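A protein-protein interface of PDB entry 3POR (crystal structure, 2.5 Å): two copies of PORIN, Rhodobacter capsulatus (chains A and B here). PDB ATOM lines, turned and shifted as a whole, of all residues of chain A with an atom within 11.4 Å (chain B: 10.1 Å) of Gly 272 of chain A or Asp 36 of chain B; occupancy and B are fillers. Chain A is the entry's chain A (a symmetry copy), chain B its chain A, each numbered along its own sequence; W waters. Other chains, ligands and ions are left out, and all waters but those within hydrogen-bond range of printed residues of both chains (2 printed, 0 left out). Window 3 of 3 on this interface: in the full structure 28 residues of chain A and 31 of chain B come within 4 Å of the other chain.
Water W1 bridges O of Gly 273 of chain A (2.7 Å) and N of Thr 34 of chain B (2.8 Å).
Water W2 lies within hydrogen-bond range of O of Ser 32 of chain B and O of Lys 300 of chain A.
Hydrophobic or aromatic side chains of chain B within 4 Å of the printed part of chain A: Phe 41.
Among the printed residues, no Asp or Glu carboxylate lies within 4 Å of a Lys or Arg side-chain nitrogen of the other chain.
No position is printed for both chains.
The backbone NH (N) of Phe 41 of chain B lies within hydrogen-bond range of the backbone carbonyl oxygen (O) of Gly 33 of chain B (3.1 Å).
OD1 of Asp 270 of chain A is in hydrogen-bond range of N of Gly 272 of chain A.
N of Lys 300 of chain A sits at hydrogen-bond distance from O of Gly 274 of chain A.
The backbone NH (N) of Leu 39 of chain B sits at hydrogen-bond distance from the side-chain hydroxyl (OG1) of Thr 35 of chain B.
OG1 of Thr 34 of chain B is in hydrogen-bond range of OE1 of Glu 40 of chain B.
CB of Thr 35 of chain B touches O of Leu 271 of chain A, at 3.5 Å.
Gly 272 of chain A touches Thr 35 of chain B (O to CA, 3.5 Å).
Gly 272 of chain A touches Asp 36 of chain B.
Gly 273 of chain A touches Thr 34 of chain B (CA to O, 3.6 Å).
O of Gly 273 of chain A touches CZ of Phe 41 of chain B, at 3.4 Å.
Gly 274 of chain A touches Phe 41 of chain B (C to CZ, 3.9 Å).
Thr 35 of chain B touches Ala 275 of chain A (CG2 to CB, 3.7 Å).
CD1 of Phe 41 of chain B touches CG of Phe 299 of chain A, at 3.6 Å.
Phe 301 of chain A touches Ser 32 of chain B (CD1 to O, 3.4 Å).
CE1 of Phe 41 of chain B touches CE1 of Phe 301 of chain A, 3.5 Å away.
The backbone NH (N) of Asp 36 of chain B is in hydrogen-bond range of the backbone carbonyl oxygen (O) of Leu 271 of chain A, 3.1 Å away.
Gly 272 of chain A touches two residues of chain B.
Asp 36 of chain B touches two residues of chain A.
Leu 271 of chain A touches just these residues of chain B: Thr 35 (3.5 Å) and Asp 36 (3.1 Å).
Gly 273 of chain A touches two residues of chain B.
Gly 274 of chain A touches just one residue of chain B: Phe 41.
Of chain B, only Thr 35 (3.7 Å) and Phe 41 (3.6 Å) come within 4 Å of Ala 275 of chain A.
Of the printed residues of chain A, Thr 34 of chain B touches Gly 273 (3.6 Å).
Printed residues of chain A within 4 Å of Thr 35 of chain B: Leu 271 (3.5 Å), Gly 272 (3.5 Å) and Ala 275 (3.7 Å).
No residue of chain A comes within 4 Å of Ser 37 of chain B.
Of the printed residues of chain B, Phe 301 of chain A touches Ser 32 and Phe 41.
Of the printed residues of chain A, Ser 32 of chain B touches Phe 301 (3.4 Å).
Of the printed residues of chain A, Phe 41 of chain B touches Gly 273 (3.4 Å), Gly 274 (3.9 Å), Ala 275 (3.6 Å), Phe 299 (3.6 Å) and Phe 301 (3.5 Å).
Printed residues of chain B within 4 Å of Phe 299 of chain A: Phe 41.
The nearest residue of chain B that does not touch Gly 272 of chain A is Thr 34 of chain B (4.3 Å).
The nearest residue of chain A that does not touch Asp 36 of chain B is Gly 273 of chain A (4.4 Å).
The nearest printed residue of chain B that does not touch Phe 299 of chain A is Leu 63 of chain B (4.2 Å).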
ATOM      1  N   GLY A 241      17.233  11.238  27.516  1.00  0.00           N
ATOM      2  CA  GLY A 241      16.412  11.773  26.501  1.00  0.00           C
ATOM      3  C   GLY A 241      15.068  11.191  26.778  1.00  0.00           C
ATOM      4  O   GLY A 241      14.466  11.496  27.828  1.00  0.00           O
ATOM      5  N   ALA A 242      14.674  10.355  25.819  1.00  0.00           N
ATOM      6  CA  ALA A 242      13.396   9.679  25.907  1.00  0.00           C
ATOM      7  C   ALA A 242      13.555   8.221  26.295  1.00  0.00           C
ATOM      8  O   ALA A 242      12.534   7.533  26.359  1.00  0.00           O
ATOM      9  CB  ALA A 242      12.674   9.704  24.589  1.00  0.00           C
ATOM     10  N   THR A 243      14.764   7.735  26.579  1.00  0.00           N
ATOM     11  CA  THR A 243      14.961   6.379  26.963  1.00  0.00           C
ATOM     12  C   THR A 243      15.339   6.271  28.417  1.00  0.00           C
ATOM     13  O   THR A 243      16.274   6.945  28.837  1.00  0.00           O
ATOM     14  CB  THR A 243      16.037   5.798  26.109  1.00  0.00           C
ATOM     15  OG1 THR A 243      15.697   6.153  24.781  1.00  0.00           O
ATOM     16  CG2 THR A 243      16.072   4.263  26.126  1.00  0.00           C
ATOM     17  N   THR A 244      14.603   5.476  29.202  1.00  0.00           N
ATOM     18  CA  THR A 244      14.924   5.182  30.578  1.00  0.00           C
ATOM     19  C   THR A 244      15.392   3.765  30.625  1.00  0.00           C
ATOM     20  O   THR A 244      14.815   2.924  29.956  1.00  0.00           O
ATOM     21  CB  THR A 244      13.748   5.277  31.412  1.00  0.00           C
ATOM     22  OG1 THR A 244      13.379   6.628  31.286  1.00  0.00           O
ATOM     23  CG2 THR A 244      13.975   4.911  32.844  1.00  0.00           C
ATOM     24  N   SER A 268      12.209   1.844  28.660  1.00  0.00           N
ATOM     25  CA  SER A 268      11.006   2.471  28.125  1.00  0.00           C
ATOM     26  C   SER A 268      11.504   3.455  27.099  1.00  0.00           C
ATOM     27  O   SER A 268      12.578   4.049  27.277  1.00  0.00           O
ATOM     28  CB  SER A 268      10.247   3.428  28.982  1.00  0.00           C
ATOM     29  OG  SER A 268      10.012   3.225  30.352  1.00  0.00           O
ATOM     30  N   TYR A 269      10.691   3.701  26.095  1.00  0.00           N
ATOM     31  CA  TYR A 269      10.973   4.732  25.164  1.00  0.00           C
ATOM     32  C   TYR A 269       9.718   5.555  25.118  1.00  0.00           C
ATOM     33  O   TYR A 269       8.668   5.021  24.747  1.00  0.00           O
ATOM     34  CB  TYR A 269      11.256   4.118  23.849  1.00  0.00           C
ATOM     35  CG  TYR A 269      11.706   5.219  22.915  1.00  0.00           C
ATOM     36  CD1 TYR A 269      12.943   5.808  23.092  1.00  0.00           C
ATOM     37  CD2 TYR A 269      10.854   5.664  21.934  1.00  0.00           C
ATOM     38  CE1 TYR A 269      13.318   6.853  22.283  1.00  0.00           C
ATOM     39  CE2 TYR A 269      11.234   6.715  21.132  1.00  0.00           C
ATOM     40  CZ  TYR A 269      12.461   7.310  21.307  1.00  0.00           C
ATOM     41  OH  TYR A 269      12.813   8.399  20.518  1.00  0.00           O
ATOM     42  N   ASP A 270       9.792   6.843  25.414  1.00  0.00           N
ATOM     43  CA  ASP A 270       8.619   7.679  25.445  1.00  0.00           C
ATOM     44  C   ASP A 270       8.152   8.172  24.108  1.00  0.00           C
ATOM     45  O   ASP A 270       8.812   9.015  23.541  1.00  0.00           O
ATOM     46  CB  ASP A 270       8.914   8.841  26.315  1.00  0.00           C
ATOM     47  CG  ASP A 270       7.751   9.734  26.746  1.00  0.00           C
ATOM     48  OD1 ASP A 270       6.711   9.692  26.109  1.00  0.00           O
ATOM     49  OD2 ASP A 270       7.885  10.485  27.734  1.00  0.00           O
ATOM     50  N   LEU A 271       7.016   7.811  23.562  1.00  0.00           N
ATOM     51  CA  LEU A 271       6.617   8.365  22.280  1.00  0.00           C
ATOM     52  C   LEU A 271       5.983   9.774  22.401  1.00  0.00           C
ATOM     53  O   LEU A 271       5.490  10.427  21.479  1.00  0.00           O
ATOM     54  CB  LEU A 271       5.666   7.394  21.708  1.00  0.00           C
ATOM     55  CG  LEU A 271       6.126   5.993  21.557  1.00  0.00           C
ATOM     56  CD1 LEU A 271       4.973   5.059  21.215  1.00  0.00           C
ATOM     57  CD2 LEU A 271       7.123   5.994  20.464  1.00  0.00           C
ATOM     58  N   GLY A 272       5.904  10.243  23.612  1.00  0.00           N
ATOM     59  CA  GLY A 272       5.303  11.495  23.925  1.00  0.00           C
ATOM     60  C   GLY A 272       3.802  11.371  23.937  1.00  0.00           C
ATOM     61  O   GLY A 272       3.291  10.462  23.328  1.00  0.00           O
ATOM     62  N   GLY A 273       2.982  12.139  24.648  1.00  0.00           N
ATOM     63  CA  GLY A 273       1.550  12.133  24.419  1.00  0.00           C
ATOM     64  C   GLY A 273       0.797  11.195  25.344  1.00  0.00           C
ATOM     65  O   GLY A 273      -0.451  11.191  25.369  1.00  0.00           O
ATOM     66  N   GLY A 274       1.547  10.393  26.109  1.00  0.00           N
ATOM     67  CA  GLY A 274       0.970   9.473  27.044  1.00  0.00           C
ATOM     68  C   GLY A 274       1.277   8.051  26.626  1.00  0.00           C
ATOM     69  O   GLY A 274       0.819   7.177  27.359  1.00  0.00           O
ATOM     70  N   ALA A 275       1.967   7.759  25.508  1.00  0.00           N
ATOM     71  CA  ALA A 275       2.269   6.403  25.074  1.00  0.00           C
ATOM     72  C   ALA A 275       3.760   6.151  25.245  1.00  0.00           C
ATOM     73  O   ALA A 275       4.538   7.099  25.243  1.00  0.00           O
ATOM     74  CB  ALA A 275       1.917   6.243  23.621  1.00  0.00           C
ATOM     75  N   SER A 276       4.280   4.963  25.499  1.00  0.00           N
ATOM     76  CA  SER A 276       5.713   4.669  25.509  1.00  0.00           C
ATOM     77  C   SER A 276       5.826   3.197  25.224  1.00  0.00           C
ATOM     78  O   SER A 276       4.813   2.518  25.412  1.00  0.00           O
ATOM     79  CB  SER A 276       6.326   4.903  26.806  1.00  0.00           C
ATOM     80  OG  SER A 276       5.338   4.445  27.677  1.00  0.00           O
ATOM     81  N   ILE A 277       6.951   2.737  24.711  1.00  0.00           N
ATOM     82  CA  ILE A 277       7.172   1.341  24.436  1.00  0.00           C
ATOM     83  C   ILE A 277       7.979   0.868  25.609  1.00  0.00           C
ATOM     84  O   ILE A 277       8.957   1.517  25.989  1.00  0.00           O
ATOM     85  CB  ILE A 277       7.952   1.211  23.192  1.00  0.00           C
ATOM     86  CG1 ILE A 277       7.126   1.824  22.109  1.00  0.00           C
ATOM     87  CG2 ILE A 277       8.133  -0.224  22.785  1.00  0.00           C
ATOM     88  CD1 ILE A 277       8.103   2.276  21.040  1.00  0.00           C
ATOM     89  N   VAL A 278       7.600  -0.233  26.224  1.00  0.00           N
ATOM     90  CA  VAL A 278       8.212  -0.634  27.470  1.00  0.00           C
ATOM     91  C   VAL A 278       8.454  -2.085  27.272  1.00  0.00           C
ATOM     92  O   VAL A 278       7.623  -2.766  26.665  1.00  0.00           O
ATOM     93  CB  VAL A 278       7.233  -0.438  28.639  1.00  0.00           C
ATOM     94  CG1 VAL A 278       7.962  -0.494  29.984  1.00  0.00           C
ATOM     95  CG2 VAL A 278       6.565   0.917  28.536  1.00  0.00           C
ATOM     96  N   VAL A 297       3.185  -1.683  24.528  1.00  0.00           N
ATOM     97  CA  VAL A 297       3.043  -0.259  24.657  1.00  0.00           C
ATOM     98  C   VAL A 297       2.187   0.031  25.855  1.00  0.00           C
ATOM     99  O   VAL A 297       1.327  -0.772  26.161  1.00  0.00           O
ATOM    100  CB  VAL A 297       2.409   0.329  23.407  1.00  0.00           C
ATOM    101  CG1 VAL A 297       3.381   0.304  22.289  1.00  0.00           C
ATOM    102  CG2 VAL A 297       1.274  -0.505  22.920  1.00  0.00           C
ATOM    103  N   LYS A 298       2.321   1.145  26.532  1.00  0.00           N
ATOM    104  CA  LYS A 298       1.611   1.460  27.743  1.00  0.00           C
ATOM    105  C   LYS A 298       1.052   2.867  27.431  1.00  0.00           C
ATOM    106  O   LYS A 298       1.715   3.607  26.701  1.00  0.00           O
ATOM    107  CB  LYS A 298       2.740   1.324  28.715  1.00  0.00           C
ATOM    108  CG  LYS A 298       2.418   0.955  30.124  1.00  0.00           C
ATOM    109  CD  LYS A 298       3.681   0.730  30.849  1.00  0.00           C
ATOM    110  CE  LYS A 298       3.545   1.227  32.306  1.00  0.00           C
ATOM    111  NZ  LYS A 298       4.729   0.966  33.133  1.00  0.00           N
ATOM    112  N   PHE A 299      -0.142   3.331  27.862  1.00  0.00           N
ATOM    113  CA  PHE A 299      -0.872   4.512  27.404  1.00  0.00           C
ATOM    114  C   PHE A 299      -1.477   5.110  28.612  1.00  0.00           C
ATOM    115  O   PHE A 299      -1.935   4.359  29.433  1.00  0.00           O
ATOM    116  CB  PHE A 299      -2.008   4.172  26.585  1.00  0.00           C
ATOM    117  CG  PHE A 299      -1.735   3.497  25.253  1.00  0.00           C
ATOM    118  CD1 PHE A 299      -0.621   3.780  24.519  1.00  0.00           C
ATOM    119  CD2 PHE A 299      -2.662   2.578  24.769  1.00  0.00           C
ATOM    120  CE1 PHE A 299      -0.457   3.126  23.310  1.00  0.00           C
ATOM    121  CE2 PHE A 299      -2.491   1.930  23.565  1.00  0.00           C
ATOM    122  CZ  PHE A 299      -1.375   2.209  22.834  1.00  0.00           C
ATOM    123  N   LYS A 300      -1.522   6.407  28.812  1.00  0.00           N
ATOM    124  CA  LYS A 300      -2.067   7.033  30.015  1.00  0.00           C
ATOM    125  C   LYS A 300      -3.115   7.992  29.442  1.00  0.00           C
ATOM    126  O   LYS A 300      -2.778   8.587  28.408  1.00  0.00           O
ATOM    127  CB  LYS A 300      -0.959   7.778  30.676  1.00  0.00           C
ATOM    128  CG  LYS A 300      -0.282   7.237  31.928  1.00  0.00           C
ATOM    129  CD  LYS A 300      -1.324   6.992  33.096  1.00  0.00           C
ATOM    130  CE  LYS A 300      -2.426   8.084  33.501  1.00  0.00           C
ATOM    131  NZ  LYS A 300      -3.544   7.537  34.292  1.00  0.00           N
ATOM    132  N   PHE A 301      -4.358   8.145  29.911  1.00  0.00           N
ATOM    133  CA  PHE A 301      -5.319   9.022  29.301  1.00  0.00           C
ATOM    134  C   PHE A 301      -5.889   9.891  30.422  1.00  0.00           C
ATOM    135  O   PHE A 301      -5.567   9.715  31.601  1.00  0.00           O
ATOM    136  CB  PHE A 301      -6.465   8.302  28.707  1.00  0.00           C
ATOM    137  CG  PHE A 301      -6.082   7.146  27.827  1.00  0.00           C
ATOM    138  CD1 PHE A 301      -5.836   7.347  26.506  1.00  0.00           C
ATOM    139  CD2 PHE A 301      -5.995   5.874  28.364  1.00  0.00           C
ATOM    140  CE1 PHE A 301      -5.501   6.266  25.734  1.00  0.00           C
ATOM    141  CE2 PHE A 301      -5.652   4.794  27.575  1.00  0.00           C
ATOM    142  CZ  PHE A 301      -5.403   4.983  26.251  1.00  0.00           C
ATOM    143  OXT PHE A 301      -6.663  10.803  30.148  1.00  0.00           O
ATOM    144  N   SER B  32      -8.650   8.469  24.455  1.00  0.00           N
ATOM    145  CA  SER B  32      -7.778   8.729  23.253  1.00  0.00           C
ATOM    146  C   SER B  32      -6.563   9.597  23.548  1.00  0.00           C
ATOM    147  O   SER B  32      -6.473  10.177  24.667  1.00  0.00           O
ATOM    148  CB  SER B  32      -8.587   9.380  22.140  1.00  0.00           C
ATOM    149  OG  SER B  32      -9.494  10.247  22.805  1.00  0.00           O
ATOM    150  N   GLY B  33      -5.595   9.567  22.619  1.00  0.00           N
ATOM    151  CA  GLY B  33      -4.336  10.293  22.709  1.00  0.00           C
ATOM    152  C   GLY B  33      -3.583  10.233  21.370  1.00  0.00           C
ATOM    153  O   GLY B  33      -3.913   9.370  20.526  1.00  0.00           O
ATOM    154  N   THR B  34      -2.637  11.159  21.095  1.00  0.00           N
ATOM    155  CA  THR B  34      -1.876  11.196  19.859  1.00  0.00           C
ATOM    156  C   THR B  34      -0.452  11.211  20.296  1.00  0.00           C
ATOM    157  O   THR B  34      -0.209  11.928  21.251  1.00  0.00           O
ATOM    158  CB  THR B  34      -2.056  12.432  19.130  1.00  0.00           C
ATOM    159  OG1 THR B  34      -3.415  12.550  18.858  1.00  0.00           O
ATOM    160  CG2 THR B  34      -1.436  12.379  17.799  1.00  0.00           C
ATOM    161  N   THR B  35       0.492  10.463  19.736  1.00  0.00           N
ATOM    162  CA  THR B  35       1.861  10.578  20.158  1.00  0.00           C
ATOM    163  C   THR B  35       2.490  11.776  19.386  1.00  0.00           C
ATOM    164  O   THR B  35       1.920  12.298  18.405  1.00  0.00           O
ATOM    165  CB  THR B  35       2.590   9.280  19.848  1.00  0.00           C
ATOM    166  OG1 THR B  35       2.793   9.176  18.437  1.00  0.00           O
ATOM    167  CG2 THR B  35       1.783   8.098  20.386  1.00  0.00           C
ATOM    168  N   ASP B  36       3.698  12.235  19.751  1.00  0.00           N
ATOM    169  CA  ASP B  36       4.431  13.270  19.055  1.00  0.00           C
ATOM    170  C   ASP B  36       4.515  12.968  17.556  1.00  0.00           C
ATOM    171  O   ASP B  36       4.340  13.964  16.870  1.00  0.00           O
ATOM    172  CB  ASP B  36       5.835  13.389  19.679  1.00  0.00           C
ATOM    173  CG  ASP B  36       5.882  13.894  21.115  1.00  0.00           C
ATOM    174  OD1 ASP B  36       4.917  14.564  21.502  1.00  0.00           O
ATOM    175  OD2 ASP B  36       6.871  13.632  21.826  1.00  0.00           O
ATOM    176  N   SER B  37       4.665  11.790  16.919  1.00  0.00           N
ATOM    177  CA  SER B  37       4.673  11.727  15.494  1.00  0.00           C
ATOM    178  C   SER B  37       3.293  11.513  14.928  1.00  0.00           C
ATOM    179  O   SER B  37       3.138  11.223  13.735  1.00  0.00           O
ATOM    180  CB  SER B  37       5.571  10.633  15.076  1.00  0.00           C
ATOM    181  OG  SER B  37       5.205   9.341  15.564  1.00  0.00           O
ATOM    182  N   GLY B  38       2.222  11.591  15.707  1.00  0.00           N
ATOM    183  CA  GLY B  38       0.902  11.497  15.116  1.00  0.00           C
ATOM    184  C   GLY B  38       0.325  10.119  15.013  1.00  0.00           C
ATOM    185  O   GLY B  38      -0.634   9.902  14.266  1.00  0.00           O
ATOM    186  N   LEU B  39       0.901   9.194  15.777  1.00  0.00           N
ATOM    187  CA  LEU B  39       0.258   7.900  15.973  1.00  0.00           C
ATOM    188  C   LEU B  39      -0.930   8.078  16.900  1.00  0.00           C
ATOM    189  O   LEU B  39      -0.824   8.849  17.841  1.00  0.00           O
ATOM    190  CB  LEU B  39       1.146   6.967  16.624  1.00  0.00           C
ATOM    191  CG  LEU B  39       2.393   6.651  15.903  1.00  0.00           C
ATOM    192  CD1 LEU B  39       2.826   5.369  16.494  1.00  0.00           C
ATOM    193  CD2 LEU B  39       2.221   6.323  14.445  1.00  0.00           C
ATOM    194  N   GLU B  40      -2.076   7.458  16.714  1.00  0.00           N
ATOM    195  CA  GLU B  40      -3.259   7.557  17.576  1.00  0.00           C
ATOM    196  C   GLU B  40      -3.331   6.297  18.428  1.00  0.00           C
ATOM    197  O   GLU B  40      -2.917   5.183  18.028  1.00  0.00           O
ATOM    198  CB  GLU B  40      -4.517   7.586  16.775  1.00  0.00           C
ATOM    199  CG  GLU B  40      -4.592   8.588  15.624  1.00  0.00           C
ATOM    200  CD  GLU B  40      -4.496  10.010  16.165  1.00  0.00           C
ATOM    201  OE1 GLU B  40      -5.206  10.295  17.147  1.00  0.00           O
ATOM    202  OE2 GLU B  40      -3.714  10.816  15.626  1.00  0.00           O
ATOM    203  N   PHE B  41      -3.874   6.410  19.598  1.00  0.00           N
ATOM    204  CA  PHE B  41      -3.930   5.263  20.436  1.00  0.00           C
ATOM    205  C   PHE B  41      -5.151   5.457  21.268  1.00  0.00           C
ATOM    206  O   PHE B  41      -5.623   6.576  21.430  1.00  0.00           O
ATOM    207  CB  PHE B  41      -2.643   5.169  21.274  1.00  0.00           C
ATOM    208  CG  PHE B  41      -2.246   6.262  22.256  1.00  0.00           C
ATOM    209  CD1 PHE B  41      -2.856   6.381  23.479  1.00  0.00           C
ATOM    210  CD2 PHE B  41      -1.275   7.167  21.904  1.00  0.00           C
ATOM    211  CE1 PHE B  41      -2.517   7.386  24.348  1.00  0.00           C
ATOM    212  CE2 PHE B  41      -0.940   8.171  22.764  1.00  0.00           C
ATOM    213  CZ  PHE B  41      -1.559   8.279  23.988  1.00  0.00           C
ATOM    214  N   LEU B  63      -3.651   1.059  18.537  1.00  0.00           N
ATOM    215  CA  LEU B  63      -2.575   1.922  18.163  1.00  0.00           C
ATOM    216  C   LEU B  63      -2.694   1.907  16.670  1.00  0.00           C
ATOM    217  O   LEU B  63      -2.748   0.795  16.139  1.00  0.00           O
ATOM    218  CB  LEU B  63      -1.255   1.370  18.466  1.00  0.00           C
ATOM    219  CG  LEU B  63      -0.073   2.281  18.143  1.00  0.00           C
ATOM    220  CD1 LEU B  63       0.110   3.518  19.090  1.00  0.00           C
ATOM    221  CD2 LEU B  63       1.131   1.423  18.302  1.00  0.00           C
HETATM  222  O   HOH W   1      -2.212  12.159  23.623  1.00  0.00           O
HETATM  223  O   HOH W   2      -4.014  10.933  26.387  1.00  0.00           O
